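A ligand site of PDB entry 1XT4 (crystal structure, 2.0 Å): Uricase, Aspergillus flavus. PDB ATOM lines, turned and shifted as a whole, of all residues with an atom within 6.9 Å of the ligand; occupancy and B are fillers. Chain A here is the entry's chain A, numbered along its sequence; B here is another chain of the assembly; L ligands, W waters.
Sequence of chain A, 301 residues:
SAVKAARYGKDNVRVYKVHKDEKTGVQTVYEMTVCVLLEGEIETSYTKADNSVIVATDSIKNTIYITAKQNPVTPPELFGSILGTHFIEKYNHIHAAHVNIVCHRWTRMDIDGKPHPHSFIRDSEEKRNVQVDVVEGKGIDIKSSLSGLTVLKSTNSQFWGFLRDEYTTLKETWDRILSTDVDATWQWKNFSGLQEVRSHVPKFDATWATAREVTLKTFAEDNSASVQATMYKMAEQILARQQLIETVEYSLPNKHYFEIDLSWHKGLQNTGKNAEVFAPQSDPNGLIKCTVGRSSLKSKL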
ATOM      1  N   SER A 157      33.608  14.707 -29.626  1.00  0.00           N
ATOM      2  CA  SER A 157      33.040  15.869 -29.006  1.00  0.00           C
ATOM      3  C   SER A 157      31.559  15.584 -29.013  1.00  0.00           C
ATOM      4  O   SER A 157      31.038  15.014 -29.968  1.00  0.00           O
ATOM      5  CB  SER A 157      33.354  17.147 -29.767  1.00  0.00           C
ATOM      6  OG  SER A 157      32.519  18.186 -29.303  1.00  0.00           O
ATOM      7  N   GLN A 158      30.911  15.875 -27.898  1.00  0.00           N
ATOM      8  CA  GLN A 158      29.504  15.572 -27.790  1.00  0.00           C
ATOM      9  C   GLN A 158      28.823  16.764 -27.210  1.00  0.00           C
ATOM     10  O   GLN A 158      29.459  17.607 -26.615  1.00  0.00           O
ATOM     11  CB  GLN A 158      29.314  14.413 -26.781  1.00  0.00           C
ATOM     12  CG  GLN A 158      30.060  13.133 -27.180  1.00  0.00           C
ATOM     13  CD  GLN A 158      29.825  11.983 -26.198  1.00  0.00           C
ATOM     14  OE1 GLN A 158      28.748  11.851 -25.615  1.00  0.00           O
ATOM     15  NE2 GLN A 158      30.849  11.179 -25.981  1.00  0.00           N
ATOM     16  N   PHE A 159      27.494  16.757 -27.348  1.00  0.00           N
ATOM     17  CA  PHE A 159      26.681  17.742 -26.682  1.00  0.00           C
ATOM     18  C   PHE A 159      25.263  17.215 -26.540  1.00  0.00           C
ATOM     19  O   PHE A 159      24.496  17.255 -27.508  1.00  0.00           O
ATOM     20  CB  PHE A 159      26.711  19.136 -27.354  1.00  0.00           C
ATOM     21  CG  PHE A 159      26.161  20.230 -26.469  1.00  0.00           C
ATOM     22  CD1 PHE A 159      26.732  20.473 -25.226  1.00  0.00           C
ATOM     23  CD2 PHE A 159      25.026  20.925 -26.822  1.00  0.00           C
ATOM     24  CE1 PHE A 159      26.233  21.478 -24.395  1.00  0.00           C
ATOM     25  CE2 PHE A 159      24.495  21.905 -25.983  1.00  0.00           C
ATOM     26  CZ  PHE A 159      25.101  22.186 -24.759  1.00  0.00           C
ATOM     27  N   PHE A 162      21.175  18.873 -22.525  1.00  0.00           N
ATOM     28  CA  PHE A 162      20.958  20.274 -22.227  1.00  0.00           C
ATOM     29  C   PHE A 162      19.452  20.524 -22.054  1.00  0.00           C
ATOM     30  O   PHE A 162      18.633  19.735 -22.498  1.00  0.00           O
ATOM     31  CB  PHE A 162      21.548  21.147 -23.340  1.00  0.00           C
ATOM     32  CG  PHE A 162      21.162  20.706 -24.727  1.00  0.00           C
ATOM     33  CD1 PHE A 162      21.987  19.884 -25.471  1.00  0.00           C
ATOM     34  CD2 PHE A 162      19.940  21.111 -25.283  1.00  0.00           C
ATOM     35  CE1 PHE A 162      21.620  19.459 -26.746  1.00  0.00           C
ATOM     36  CE2 PHE A 162      19.592  20.745 -26.603  1.00  0.00           C
ATOM     37  CZ  PHE A 162      20.433  19.917 -27.314  1.00  0.00           C
ATOM     38  N   LEU A 170      17.513  22.517 -31.340  1.00  0.00           N
ATOM     39  CA  LEU A 170      18.801  21.837 -31.465  1.00  0.00           C
ATOM     40  C   LEU A 170      18.681  20.347 -31.059  1.00  0.00           C
ATOM     41  O   LEU A 170      18.065  20.011 -30.041  1.00  0.00           O
ATOM     42  CB  LEU A 170      19.836  22.545 -30.605  1.00  0.00           C
ATOM     43  CG  LEU A 170      21.271  21.933 -30.615  1.00  0.00           C
ATOM     44  CD1 LEU A 170      21.939  21.884 -32.008  1.00  0.00           C
ATOM     45  CD2 LEU A 170      22.232  22.499 -29.535  1.00  0.00           C
ATOM     46  N   ARG A 176      30.420  15.130 -32.905  1.00  0.00           N
ATOM     47  CA  ARG A 176      30.402  16.384 -33.670  1.00  0.00           C
ATOM     48  C   ARG A 176      31.800  16.949 -33.809  1.00  0.00           C
ATOM     49  O   ARG A 176      32.755  16.513 -33.115  1.00  0.00           O
ATOM     50  CB  ARG A 176      29.482  17.436 -33.017  1.00  0.00           C
ATOM     51  CG  ARG A 176      30.086  18.058 -31.730  1.00  0.00           C
ATOM     52  CD  ARG A 176      29.162  19.065 -31.031  1.00  0.00           C
ATOM     53  NE  ARG A 176      29.829  19.538 -29.821  1.00  0.00           N
ATOM     54  CZ  ARG A 176      29.504  20.624 -29.137  1.00  0.00           C
ATOM     55  NH1 ARG A 176      28.440  21.327 -29.481  1.00  0.00           N
ATOM     56  NH2 ARG A 176      30.260  20.985 -28.104  1.00  0.00           N
ATOM     57  N   LEU A 178      34.387  19.928 -33.300  1.00  0.00           N
ATOM     58  CA  LEU A 178      34.550  20.987 -32.309  1.00  0.00           C
ATOM     59  C   LEU A 178      35.685  21.831 -32.863  1.00  0.00           C
ATOM     60  O   LEU A 178      36.786  21.321 -33.126  1.00  0.00           O
ATOM     61  CB  LEU A 178      34.951  20.411 -30.936  1.00  0.00           C
ATOM     62  CG  LEU A 178      35.131  21.442 -29.788  1.00  0.00           C
ATOM     63  CD1 LEU A 178      33.895  22.297 -29.716  1.00  0.00           C
ATOM     64  CD2 LEU A 178      35.416  20.815 -28.395  1.00  0.00           C
ATOM     65  N   SER A 224      35.120  15.386 -25.177  1.00  0.00           N
ATOM     66  CA  SER A 224      34.438  16.582 -24.689  1.00  0.00           C
ATOM     67  C   SER A 224      32.942  16.446 -24.511  1.00  0.00           C
ATOM     68  O   SER A 224      32.225  16.092 -25.427  1.00  0.00           O
ATOM     69  CB  SER A 224      34.806  17.801 -25.558  1.00  0.00           C
ATOM     70  OG  SER A 224      34.090  18.951 -25.150  1.00  0.00           O
ATOM     71  N   ALA A 225      32.487  16.734 -23.298  1.00  0.00           N
ATOM     72  CA  ALA A 225      31.069  16.697 -22.968  1.00  0.00           C
ATOM     73  C   ALA A 225      30.397  18.042 -23.349  1.00  0.00           C
ATOM     74  O   ALA A 225      29.175  18.143 -23.514  1.00  0.00           O
ATOM     75  CB  ALA A 225      30.926  16.423 -21.483  1.00  0.00           C
ATOM     76  N   SER A 226      31.239  19.072 -23.477  1.00  0.00           N
ATOM     77  CA  SER A 226      30.807  20.439 -23.816  1.00  0.00           C
ATOM     78  C   SER A 226      32.054  21.319 -23.819  1.00  0.00           C
ATOM     79  O   SER A 226      33.113  20.924 -23.318  1.00  0.00           O
ATOM     80  CB  SER A 226      29.801  20.993 -22.793  1.00  0.00           C
ATOM     81  OG  SER A 226      30.453  21.249 -21.560  1.00  0.00           O
ATOM     82  N   VAL A 227      31.945  22.500 -24.406  1.00  0.00           N
ATOM     83  CA  VAL A 227      33.078  23.422 -24.390  1.00  0.00           C
ATOM     84  C   VAL A 227      33.362  23.809 -22.929  1.00  0.00           C
ATOM     85  O   VAL A 227      34.495  23.784 -22.510  1.00  0.00           O
ATOM     86  CB  VAL A 227      32.805  24.692 -25.264  1.00  0.00           C
ATOM     87  CG1 VAL A 227      33.981  25.618 -25.151  1.00  0.00           C
ATOM     88  CG2 VAL A 227      32.634  24.248 -26.743  1.00  0.00           C
ATOM     89  N   GLN A 228      32.303  24.021 -22.170  1.00  0.00           N
ATOM     90  CA  GLN A 228      32.389  24.382 -20.745  1.00  0.00           C
ATOM     91  C   GLN A 228      33.267  23.406 -19.949  1.00  0.00           C
ATOM     92  O   GLN A 228      34.144  23.793 -19.177  1.00  0.00           O
ATOM     93  CB  GLN A 228      30.972  24.407 -20.147  1.00  0.00           C
ATOM     94  CG  GLN A 228      30.043  25.652 -20.503  1.00  0.00           C
ATOM     95  CD  GLN A 228      29.186  25.457 -21.772  1.00  0.00           C
ATOM     96  OE1 GLN A 228      29.520  24.652 -22.629  1.00  0.00           O
ATOM     97  NE2 GLN A 228      28.149  26.275 -21.942  1.00  0.00           N
ATOM     98  N   ALA A 229      33.047  22.120 -20.180  1.00  0.00           N
ATOM     99  CA  ALA A 229      33.693  21.066 -19.419  1.00  0.00           C
ATOM    100  C   ALA A 229      35.134  20.937 -19.808  1.00  0.00           C
ATOM    101  O   ALA A 229      35.987  20.770 -18.956  1.00  0.00           O
ATOM    102  CB  ALA A 229      32.946  19.738 -19.609  1.00  0.00           C
ATOM    103  N   ASN A 254      32.471  28.932 -30.246  1.00  0.00           N
ATOM    104  CA  ASN A 254      32.193  27.605 -30.735  1.00  0.00           C
ATOM    105  C   ASN A 254      31.829  27.846 -32.207  1.00  0.00           C
ATOM    106  O   ASN A 254      30.773  28.397 -32.502  1.00  0.00           O
ATOM    107  CB  ASN A 254      31.021  27.012 -29.930  1.00  0.00           C
ATOM    108  CG  ASN A 254      30.694  25.550 -30.319  1.00  0.00           C
ATOM    109  OD1 ASN A 254      31.380  24.929 -31.116  1.00  0.00           O
ATOM    110  ND2 ASN A 254      29.598  25.037 -29.777  1.00  0.00           N
ATOM    111  N   HIS A 256      30.671  26.726 -35.559  1.00  0.00           N
ATOM    112  CA  HIS A 256      29.823  25.627 -35.992  1.00  0.00           C
ATOM    113  C   HIS A 256      30.056  25.133 -37.418  1.00  0.00           C
ATOM    114  O   HIS A 256      30.325  25.910 -38.311  1.00  0.00           O
ATOM    115  CB  HIS A 256      28.332  26.029 -35.774  1.00  0.00           C
ATOM    116  CG  HIS A 256      28.047  26.588 -34.394  1.00  0.00           C
ATOM    117  ND1 HIS A 256      28.166  25.831 -33.254  1.00  0.00           N
ATOM    118  CD2 HIS A 256      27.619  27.814 -33.994  1.00  0.00           C
ATOM    119  CE1 HIS A 256      27.797  26.558 -32.210  1.00  0.00           C
ATOM    120  NE2 HIS A 256      27.451  27.765 -32.640  1.00  0.00           N
ATOM    121  N   GLY A 286      28.621  30.358 -30.928  1.00  0.00           N
ATOM    122  CA  GLY A 286      28.527  30.246 -29.485  1.00  0.00           C
ATOM    123  C   GLY A 286      29.759  30.969 -28.913  1.00  0.00           C
ATOM    124  O   GLY A 286      30.810  31.043 -29.544  1.00  0.00           O
ATOM    125  N   ILE A 288      31.666  31.089 -25.158  1.00  0.00           N
ATOM    126  CA  ILE A 288      31.712  30.472 -23.841  1.00  0.00           C
ATOM    127  C   ILE A 288      32.923  30.991 -23.056  1.00  0.00           C
ATOM    128  O   ILE A 288      34.038  30.915 -23.538  1.00  0.00           O
ATOM    129  CB  ILE A 288      31.842  28.899 -23.938  1.00  0.00           C
ATOM    130  CG1 ILE A 288      30.739  28.211 -24.821  1.00  0.00           C
ATOM    131  CG2 ILE A 288      31.816  28.301 -22.512  1.00  0.00           C
ATOM    132  CD1 ILE A 288      31.133  28.008 -26.246  1.00  0.00           C
ATOM    133  N   TYR B   8      28.043  32.624 -20.828  1.00  0.00           N
ATOM    134  CA  TYR B   8      28.094  31.949 -22.106  1.00  0.00           C
ATOM    135  C   TYR B   8      26.820  32.382 -22.876  1.00  0.00           C
ATOM    136  O   TYR B   8      25.873  32.955 -22.315  1.00  0.00           O
ATOM    137  CB  TYR B   8      28.178  30.427 -21.881  1.00  0.00           C
ATOM    138  CG  TYR B   8      26.790  29.843 -21.637  1.00  0.00           C
ATOM    139  CD1 TYR B   8      26.113  30.055 -20.416  1.00  0.00           C
ATOM    140  CD2 TYR B   8      26.099  29.233 -22.673  1.00  0.00           C
ATOM    141  CE1 TYR B   8      24.789  29.649 -20.254  1.00  0.00           C
ATOM    142  CE2 TYR B   8      24.794  28.804 -22.505  1.00  0.00           C
ATOM    143  CZ  TYR B   8      24.132  29.061 -21.318  1.00  0.00           C
ATOM    144  OH  TYR B   8      22.842  28.618 -21.208  1.00  0.00           O
ATOM    145  N   GLY B   9      26.888  32.251 -24.194  1.00  0.00           N
ATOM    146  CA  GLY B   9      25.744  32.639 -24.991  1.00  0.00           C
ATOM    147  C   GLY B   9      26.025  32.655 -26.488  1.00  0.00           C
ATOM    148  O   GLY B   9      26.825  31.880 -26.997  1.00  0.00           O
ATOM    149  N   LYS B  10      25.311  33.522 -27.196  1.00  0.00           N
ATOM    150  CA  LYS B  10      25.433  33.538 -28.644  1.00  0.00           C
ATOM    151  C   LYS B  10      25.907  34.888 -29.096  1.00  0.00           C
ATOM    152  O   LYS B  10      25.408  35.916 -28.674  1.00  0.00           O
ATOM    153  CB  LYS B  10      24.128  33.111 -29.321  1.00  0.00           C
ATOM    154  CG  LYS B  10      24.277  32.736 -30.792  1.00  0.00           C
ATOM    155  CD  LYS B  10      25.126  31.461 -30.963  1.00  0.00           C
ATOM    156  CE  LYS B  10      24.467  30.412 -31.853  1.00  0.00           C
ATOM    157  NZ  LYS B  10      24.992  29.029 -31.570  1.00  0.00           N
ATOM    158  N   ASN B  51      25.034  19.197 -18.228  1.00  0.00           N
ATOM    159  CA  ASN B  51      24.454  20.078 -19.235  1.00  0.00           C
ATOM    160  C   ASN B  51      23.012  20.465 -18.977  1.00  0.00           C
ATOM    161  O   ASN B  51      22.461  21.354 -19.655  1.00  0.00           O
ATOM    162  CB  ASN B  51      24.593  19.475 -20.631  1.00  0.00           C
ATOM    163  CG  ASN B  51      26.017  19.386 -21.078  1.00  0.00           C
ATOM    164  OD1 ASN B  51      26.895  20.051 -20.520  1.00  0.00           O
ATOM    165  ND2 ASN B  51      26.279  18.585 -22.118  1.00  0.00           N
ATOM    166  N   ILE B  54      22.220  24.066 -18.838  1.00  0.00           N
ATOM    167  CA  ILE B  54      22.487  24.848 -20.048  1.00  0.00           C
ATOM    168  C   ILE B  54      21.312  25.062 -20.972  1.00  0.00           C
ATOM    169  O   ILE B  54      20.686  24.121 -21.453  1.00  0.00           O
ATOM    170  CB  ILE B  54      23.644  24.241 -20.871  1.00  0.00           C
ATOM    171  CG1 ILE B  54      24.906  24.177 -20.002  1.00  0.00           C
ATOM    172  CG2 ILE B  54      23.954  25.115 -22.115  1.00  0.00           C
ATOM    173  CD1 ILE B  54      25.963  23.287 -20.614  1.00  0.00           C
ATOM    174  N   VAL B  55      20.992  26.333 -21.162  1.00  0.00           N
ATOM    175  CA  VAL B  55      20.060  26.792 -22.181  1.00  0.00           C
ATOM    176  C   VAL B  55      20.998  26.879 -23.429  1.00  0.00           C
ATOM    177  O   VAL B  55      21.935  27.695 -23.459  1.00  0.00           O
ATOM    178  CB  VAL B  55      19.530  28.222 -21.840  1.00  0.00           C
ATOM    179  CG1 VAL B  55      18.726  28.832 -23.000  1.00  0.00           C
ATOM    180  CG2 VAL B  55      18.703  28.216 -20.524  1.00  0.00           C
ATOM    181  N   ALA B  56      20.833  25.960 -24.375  1.00  0.00           N
ATOM    182  CA  ALA B  56      21.662  25.863 -25.577  1.00  0.00           C
ATOM    183  C   ALA B  56      21.830  27.218 -26.286  1.00  0.00           C
ATOM    184  O   ALA B  56      20.868  28.005 -26.401  1.00  0.00           O
ATOM    185  CB  ALA B  56      21.086  24.797 -26.555  1.00  0.00           C
ATOM    186  N   THR B  57      23.047  27.505 -26.755  1.00  0.00           N
ATOM    187  CA  THR B  57      23.282  28.794 -27.417  1.00  0.00           C
ATOM    188  C   THR B  57      22.400  28.925 -28.666  1.00  0.00           C
ATOM    189  O   THR B  57      21.850  29.991 -28.926  1.00  0.00           O
ATOM    190  CB  THR B  57      24.746  29.040 -27.744  1.00  0.00           C
ATOM    191  OG1 THR B  57      25.183  28.122 -28.776  1.00  0.00           O
ATOM    192  CG2 THR B  57      25.596  28.822 -26.479  1.00  0.00           C
ATOM    193  N   ASP B  58      22.119  27.798 -29.300  1.00  0.00           N
ATOM    194  CA  ASP B  58      21.210  27.750 -30.430  1.00  0.00           C
ATOM    195  C   ASP B  58      19.776  28.199 -30.046  1.00  0.00           C
ATOM    196  O   ASP B  58      19.077  28.850 -30.830  1.00  0.00           O
ATOM    197  CB  ASP B  58      21.223  26.346 -31.031  1.00  0.00           C
ATOM    198  CG  ASP B  58      20.374  26.251 -32.291  1.00  0.00           C
ATOM    199  OD1 ASP B  58      20.911  26.621 -33.344  1.00  0.00           O
ATOM    200  OD2 ASP B  58      19.186  25.814 -32.238  1.00  0.00           O
ATOM    201  N   SER B  59      19.351  27.857 -28.818  1.00  0.00           N
ATOM    202  CA  SER B  59      18.033  28.284 -28.312  1.00  0.00           C
ATOM    203  C   SER B  59      18.005  29.771 -28.038  1.00  0.00           C
ATOM    204  O   SER B  59      16.972  30.409 -28.146  1.00  0.00           O
ATOM    205  CB  SER B  59      17.667  27.522 -27.008  1.00  0.00           C
ATOM    206  OG  SER B  59      17.822  26.128 -27.223  1.00  0.00           O
HETATM  207  N1  LIG L   1      25.923  23.938 -28.582  1.00  0.00           N
HETATM  208  C1  LIG L   1      24.903  24.765 -28.201  1.00  0.00           C
HETATM  209  N2  LIG L   1      25.056  25.310 -27.011  1.00  0.00           N
HETATM  210  C2  LIG L   1      26.271  24.779 -26.574  1.00  0.00           C
HETATM  211  C3  LIG L   1      26.979  25.000 -25.349  1.00  0.00           C
HETATM  212  O1  LIG L   1      26.672  25.737 -24.420  1.00  0.00           O
HETATM  213  N3  LIG L   1      28.156  24.256 -25.300  1.00  0.00           N
HETATM  214  C4  LIG L   1      28.609  23.411 -26.298  1.00  0.00           C
HETATM  215  N4  LIG L   1      29.760  22.781 -26.062  1.00  0.00           N
HETATM  216  N5  LIG L   1      27.966  23.218 -27.466  1.00  0.00           N
HETATM  217  C5  LIG L   1      26.803  23.930 -27.530  1.00  0.00           C
HETATM  218  O   HOH W   1      27.783  26.930 -28.615  1.00  0.00           O
HETATM  219  O   HOH W   2      26.085  23.019 -31.199  1.00  0.00           O
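N2 of the ligand lies within hydrogen-bond range of N of Thr 57 of chain B (3.0 Å). The side-chain amide nitrogen of Asn 254 lies within hydrogen-bond range of a nitrogen (N5) of the ligand, at 3.4 Å. The side-chain amide nitrogen (NE2) of Gln 228 is in hydrogen-bond range of an oxygen (O1) of the ligand (2.9 Å). N2 of the ligand lies within hydrogen-bond range of OG1 of Thr 57 of chain B (3.3 Å). N5 of the ligand sits at hydrogen-bond distance from NH1 of Arg 176, at 2.8 Å.
Water W2 lies within hydrogen-bond range of a nitrogen (N1) of the ligand (2.8 Å) and the guanidinium group (NH1) of Arg 176 (3.4 Å). Water W1 bridges the side-chain hydroxyl of Thr 57 of chain B and the side-chain amide nitrogen of Asn 254.
The backbone NH of Val 227 sits close to a nitrogen (N4) of the ligand, 2.8 Å away. Phe 159 touches the ligand. Leu 170 touches the ligand (CD2 to C1, 3.7 Å). Ser 226 touches the ligand (CA to N4, 3.4 Å). Tyr 8 of chain B touches the ligand. CG2 of Ile 54 of chain B touches O1 of the ligand (3.6 Å). Ala 56 of chain B touches the ligand (CA to N2, 3.7 Å). 11 residues have an atom within 4 Å of the ligand: Phe 159, Leu 170, Arg 176, Ser 226, Val 227, Gln 228, Asn 254, Tyr 8 of chain B, Ile 54 of chain B, Ala 56 of chain B and Thr 57 of chain B.
OG of Ser 226 lies within hydrogen-bond range of N of Ala 229 (3.1 Å). The side-chain hydroxyl (OH) of Tyr 8 of chain B is in hydrogen-bond range of the backbone carbonyl oxygen (O) of Val 55 of chain B. N of Asn 254 is in hydrogen-bond range of O of Gly 286, at 2.8 Å. The backbone carbonyl oxygen (O) of Ser 226 is in hydrogen-bond range of the side-chain hydroxyl (OG) of Ser 224, 2.9 Å away. The side-chain hydroxyl (OG) of Ser 226 sits close to the backbone NH (N) of Gln 228 (3.4 Å). The side-chain amino group of Lys 10 of chain B sits at hydrogen-bond distance from the side-chain hydroxyl of Thr 57 of chain B (2.9 Å). The backbone NH (N) of Arg 176 sits at hydrogen-bond distance from the backbone carbonyl oxygen (O) of Ser 157, at 3.0 Å. A ring nitrogen (NE2) of His 256 sits at hydrogen-bond distance from the backbone carbonyl oxygen (O) of Asn 254.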
